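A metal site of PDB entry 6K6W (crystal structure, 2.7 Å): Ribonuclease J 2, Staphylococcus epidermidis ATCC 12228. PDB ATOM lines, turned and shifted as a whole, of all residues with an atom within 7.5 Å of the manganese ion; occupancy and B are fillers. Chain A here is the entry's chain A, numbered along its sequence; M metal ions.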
ATOM      1  N   ASN A  39      21.419  -6.221 -22.443  1.00  0.00           N
ATOM      2  CA  ASN A  39      21.061  -7.602 -22.637  1.00  0.00           C
ATOM      3  C   ASN A  39      19.882  -7.871 -23.561  1.00  0.00           C
ATOM      4  O   ASN A  39      18.814  -7.260 -23.448  1.00  0.00           O
ATOM      5  CB  ASN A  39      20.821  -8.283 -21.282  1.00  0.00           C
ATOM      6  CG  ASN A  39      22.092  -8.390 -20.454  1.00  0.00           C
ATOM      7  OD1 ASN A  39      22.800  -9.397 -20.522  1.00  0.00           O
ATOM      8  ND2 ASN A  39      22.377  -7.361 -19.679  1.00  0.00           N
ATOM      9  N   THR A  89      13.762 -10.431 -16.989  1.00  0.00           N
ATOM     10  CA  THR A  89      14.245 -10.988 -15.729  1.00  0.00           C
ATOM     11  C   THR A  89      14.095 -10.044 -14.535  1.00  0.00           C
ATOM     12  O   THR A  89      13.745 -10.490 -13.442  1.00  0.00           O
ATOM     13  CB  THR A  89      15.725 -11.400 -15.831  1.00  0.00           C
ATOM     14  OG1 THR A  89      16.498 -10.292 -16.304  1.00  0.00           O
ATOM     15  CG2 THR A  89      15.885 -12.573 -16.778  1.00  0.00           C
ATOM     16  N   HIS A  90      14.357  -8.758 -14.739  1.00  0.00           N
ATOM     17  CA  HIS A  90      14.242  -7.785 -13.649  1.00  0.00           C
ATOM     18  C   HIS A  90      14.071  -6.355 -14.178  1.00  0.00           C
ATOM     19  O   HIS A  90      14.237  -6.101 -15.362  1.00  0.00           O
ATOM     20  CB  HIS A  90      15.472  -7.871 -12.739  1.00  0.00           C
ATOM     21  CG  HIS A  90      16.766  -7.616 -13.433  1.00  0.00           C
ATOM     22  ND1 HIS A  90      17.266  -8.456 -14.403  1.00  0.00           N
ATOM     23  CD2 HIS A  90      17.691  -6.629 -13.277  1.00  0.00           C
ATOM     24  CE1 HIS A  90      18.435  -7.989 -14.834  1.00  0.00           C
ATOM     25  NE2 HIS A  90      18.710  -6.880 -14.161  1.00  0.00           N
ATOM     26  N   GLY A  91      13.771  -5.426 -13.268  1.00  0.00           N
ATOM     27  CA  GLY A  91      13.384  -4.079 -13.669  1.00  0.00           C
ATOM     28  C   GLY A  91      14.492  -3.092 -13.975  1.00  0.00           C
ATOM     29  O   GLY A  91      14.220  -1.922 -14.260  1.00  0.00           O
ATOM     30  N   HIS A  92      15.728  -3.545 -13.951  1.00  0.00           N
ATOM     31  CA  HIS A  92      16.855  -2.686 -14.285  1.00  0.00           C
ATOM     32  C   HIS A  92      16.876  -2.279 -15.743  1.00  0.00           C
ATOM     33  O   HIS A  92      16.271  -2.926 -16.593  1.00  0.00           O
ATOM     34  CB  HIS A  92      18.172  -3.348 -13.922  1.00  0.00           C
ATOM     35  CG  HIS A  92      18.497  -3.282 -12.459  1.00  0.00           C
ATOM     36  ND1 HIS A  92      19.381  -4.151 -11.863  1.00  0.00           N
ATOM     37  CD2 HIS A  92      18.058  -2.453 -11.494  1.00  0.00           C
ATOM     38  CE1 HIS A  92      19.471  -3.846 -10.582  1.00  0.00           C
ATOM     39  NE2 HIS A  92      18.683  -2.834 -10.320  1.00  0.00           N
ATOM     40  N   GLU A  93      17.613  -1.210 -16.045  1.00  0.00           N
ATOM     41  CA  GLU A  93      17.630  -0.650 -17.390  1.00  0.00           C
ATOM     42  C   GLU A  93      18.518  -1.466 -18.331  1.00  0.00           C
ATOM     43  O   GLU A  93      18.450  -1.288 -19.545  1.00  0.00           O
ATOM     44  CB  GLU A  93      18.117   0.800 -17.348  1.00  0.00           C
ATOM     45  CG  GLU A  93      17.142   1.787 -16.702  1.00  0.00           C
ATOM     46  CD  GLU A  93      15.967   2.132 -17.586  1.00  0.00           C
ATOM     47  OE1 GLU A  93      15.063   1.280 -17.749  1.00  0.00           O
ATOM     48  OE2 GLU A  93      15.934   3.256 -18.123  1.00  0.00           O
ATOM     49  N   HIS A  94      19.339  -2.337 -17.769  1.00  0.00           N
ATOM     50  CA  HIS A  94      20.105  -3.257 -18.616  1.00  0.00           C
ATOM     51  C   HIS A  94      19.266  -4.463 -19.000  1.00  0.00           C
ATOM     52  O   HIS A  94      19.695  -5.288 -19.803  1.00  0.00           O
ATOM     53  CB  HIS A  94      21.391  -3.718 -17.930  1.00  0.00           C
ATOM     54  CG  HIS A  94      21.319  -3.784 -16.433  1.00  0.00           C
ATOM     55  ND1 HIS A  94      21.620  -2.703 -15.622  1.00  0.00           N
ATOM     56  CD2 HIS A  94      20.982  -4.795 -15.611  1.00  0.00           C
ATOM     57  CE1 HIS A  94      21.483  -3.061 -14.356  1.00  0.00           C
ATOM     58  NE2 HIS A  94      21.098  -4.321 -14.326  1.00  0.00           N
ATOM     59  N   ALA A  95      18.091  -4.593 -18.404  1.00  0.00           N
ATOM     60  CA  ALA A  95      17.192  -5.697 -18.743  1.00  0.00           C
ATOM     61  C   ALA A  95      15.963  -5.259 -19.537  1.00  0.00           C
ATOM     62  O   ALA A  95      15.532  -5.956 -20.458  1.00  0.00           O
ATOM     63  CB  ALA A  95      16.762  -6.423 -17.481  1.00  0.00           C
ATOM     64  N   HIS A 158      19.323 -10.382  -6.548  1.00  0.00           N
ATOM     65  CA  HIS A 158      19.905  -9.286  -7.304  1.00  0.00           C
ATOM     66  C   HIS A 158      19.783  -8.012  -6.479  1.00  0.00           C
ATOM     67  O   HIS A 158      19.354  -8.058  -5.332  1.00  0.00           O
ATOM     68  CB  HIS A 158      19.208  -9.156  -8.662  1.00  0.00           C
ATOM     69  CG  HIS A 158      19.985  -8.396  -9.682  1.00  0.00           C
ATOM     70  ND1 HIS A 158      21.355  -8.477  -9.801  1.00  0.00           N
ATOM     71  CD2 HIS A 158      19.587  -7.531 -10.647  1.00  0.00           C
ATOM     72  CE1 HIS A 158      21.769  -7.706 -10.791  1.00  0.00           C
ATOM     73  NE2 HIS A 158      20.708  -7.120 -11.318  1.00  0.00           N
ATOM     74  N   SER A 159      20.155  -6.871  -7.054  1.00  0.00           N
ATOM     75  CA  SER A 159      20.083  -5.622  -6.314  1.00  0.00           C
ATOM     76  C   SER A 159      18.668  -5.056  -6.312  1.00  0.00           C
ATOM     77  O   SER A 159      18.364  -4.095  -5.602  1.00  0.00           O
ATOM     78  CB  SER A 159      21.065  -4.599  -6.891  1.00  0.00           C
ATOM     79  OG  SER A 159      21.067  -4.668  -8.301  1.00  0.00           O
ATOM     80  N   ILE A 160      17.805  -5.650  -7.131  1.00  0.00           N
ATOM     81  CA  ILE A 160      16.418  -5.218  -7.265  1.00  0.00           C
ATOM     82  C   ILE A 160      15.500  -6.418  -7.006  1.00  0.00           C
ATOM     83  O   ILE A 160      15.781  -7.529  -7.468  1.00  0.00           O
ATOM     84  CB  ILE A 160      16.172  -4.603  -8.674  1.00  0.00           C
ATOM     85  CG1 ILE A 160      14.771  -3.977  -8.777  1.00  0.00           C
ATOM     86  CG2 ILE A 160      16.401  -5.610  -9.780  1.00  0.00           C
ATOM     87  CD1 ILE A 160      14.564  -3.170 -10.042  1.00  0.00           C
ATOM     88  N   GLY A 179      19.600 -14.602 -16.071  1.00  0.00           N
ATOM     89  CA  GLY A 179      19.520 -13.174 -15.908  1.00  0.00           C
ATOM     90  C   GLY A 179      20.709 -12.804 -15.034  1.00  0.00           C
ATOM     91  O   GLY A 179      21.655 -13.583 -14.919  1.00  0.00           O
ATOM     92  N   GLU A 180      20.681 -11.614 -14.452  1.00  0.00           N
ATOM     93  CA  GLU A 180      21.729 -11.235 -13.529  1.00  0.00           C
ATOM     94  C   GLU A 180      21.367 -11.750 -12.135  1.00  0.00           C
ATOM     95  O   GLU A 180      20.221 -11.615 -11.710  1.00  0.00           O
ATOM     96  CB  GLU A 180      21.939  -9.723 -13.515  1.00  0.00           C
ATOM     97  CG  GLU A 180      22.271  -9.141 -14.873  1.00  0.00           C
ATOM     98  CD  GLU A 180      22.381  -7.619 -14.833  1.00  0.00           C
ATOM     99  OE1 GLU A 180      21.823  -7.015 -13.895  1.00  0.00           O
ATOM    100  OE2 GLU A 180      23.026  -7.051 -15.734  1.00  0.00           O
ATOM    101  N   PHE A 181      22.333 -12.307 -11.426  1.00  0.00           N
ATOM    102  CA  PHE A 181      22.029 -12.982 -10.182  1.00  0.00           C
ATOM    103  C   PHE A 181      23.222 -12.989  -9.237  1.00  0.00           C
ATOM    104  O   PHE A 181      24.358 -12.730  -9.628  1.00  0.00           O
ATOM    105  CB  PHE A 181      21.571 -14.418 -10.440  1.00  0.00           C
ATOM    106  CG  PHE A 181      22.704 -15.366 -10.757  1.00  0.00           C
ATOM    107  CD1 PHE A 181      23.222 -15.449 -12.026  1.00  0.00           C
ATOM    108  CD2 PHE A 181      23.240 -16.178  -9.760  1.00  0.00           C
ATOM    109  CE1 PHE A 181      24.248 -16.320 -12.319  1.00  0.00           C
ATOM    110  CE2 PHE A 181      24.266 -17.048 -10.053  1.00  0.00           C
ATOM    111  CZ  PHE A 181      24.768 -17.115 -11.323  1.00  0.00           C
ATOM    112  N   ASP A 212      25.210 -15.113 -16.218  1.00  0.00           N
ATOM    113  CA  ASP A 212      25.855 -13.814 -16.013  1.00  0.00           C
ATOM    114  C   ASP A 212      27.360 -13.908 -15.751  1.00  0.00           C
ATOM    115  O   ASP A 212      27.778 -14.577 -14.809  1.00  0.00           O
ATOM    116  CB  ASP A 212      25.173 -13.088 -14.843  1.00  0.00           C
ATOM    117  CG  ASP A 212      25.657 -11.662 -14.654  1.00  0.00           C
ATOM    118  OD1 ASP A 212      26.488 -11.193 -15.468  1.00  0.00           O
ATOM    119  OD2 ASP A 212      25.210 -11.011 -13.696  1.00  0.00           O
ATOM    120  N   SER A 250      19.468   2.133  -9.212  1.00  0.00           N
ATOM    121  CA  SER A 250      19.286   0.729  -9.528  1.00  0.00           C
ATOM    122  C   SER A 250      19.440  -0.187  -8.306  1.00  0.00           C
ATOM    123  O   SER A 250      18.897  -1.294  -8.278  1.00  0.00           O
ATOM    124  CB  SER A 250      20.272   0.306 -10.617  1.00  0.00           C
ATOM    125  OG  SER A 250      21.614   0.428 -10.177  1.00  0.00           O
ATOM    126  N   SER A 383      26.305  -6.656  -7.628  1.00  0.00           N
ATOM    127  CA  SER A 383      24.990  -7.253  -7.840  1.00  0.00           C
ATOM    128  C   SER A 383      25.145  -8.611  -8.492  1.00  0.00           C
ATOM    129  O   SER A 383      24.196  -9.397  -8.573  1.00  0.00           O
ATOM    130  CB  SER A 383      24.101  -6.352  -8.699  1.00  0.00           C
ATOM    131  OG  SER A 383      24.194  -4.990  -8.303  1.00  0.00           O
ATOM    132  N   HIS A 384      26.352  -8.907  -8.939  1.00  0.00           N
ATOM    133  CA  HIS A 384      26.613 -10.113  -9.693  1.00  0.00           C
ATOM    134  C   HIS A 384      27.514 -11.056  -8.912  1.00  0.00           C
ATOM    135  O   HIS A 384      28.386 -10.623  -8.163  1.00  0.00           O
ATOM    136  CB  HIS A 384      27.239  -9.783 -11.044  1.00  0.00           C
ATOM    137  CG  HIS A 384      26.552  -8.668 -11.760  1.00  0.00           C
ATOM    138  ND1 HIS A 384      25.567  -8.884 -12.700  1.00  0.00           N
ATOM    139  CD2 HIS A 384      26.701  -7.318 -11.667  1.00  0.00           C
ATOM    140  CE1 HIS A 384      25.139  -7.719 -13.151  1.00  0.00           C
ATOM    141  NE2 HIS A 384      25.805  -6.753 -12.538  1.00  0.00           N
HETATM  142 MN    MN M   1      20.792  -5.677 -13.030  1.00  0.00          MN
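A ring nitrogen (NE2) of His 92 sits at hydrogen-bond distance from the backbone carbonyl oxygen of Ser 250 (2.6 Å).
The backbone carbonyl oxygen (O) of His 94 lies within hydrogen-bond range of the backbone NH (N) of Asn 39, at 3.3 Å.
ND1 of His 90 sits at hydrogen-bond distance from OG1 of Thr 89 (2.8 Å).
A ring nitrogen (ND1) of His 158 sits at hydrogen-bond distance from the backbone carbonyl oxygen (O) of Ser 383 (3.2 Å).
Within 4 Å of the manganese ion: His 90, His 92, His 94, His 158 and Glu 180.
The nearest printed residue that does not touch the manganese ion is His 384 (4.8 Å).
The manganese ion is bound by the side-chain carboxylate (OE1) of Glu 180 (1.9 Å), a ring nitrogen (NE2) of His 94 (1.9 Å), a ring nitrogen (NE2) of His 158 (2.2 Å), a ring nitrogen (ND1) of His 92 (2.4 Å) and a ring nitrogen (NE2) of His 90 (2.7 Å).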
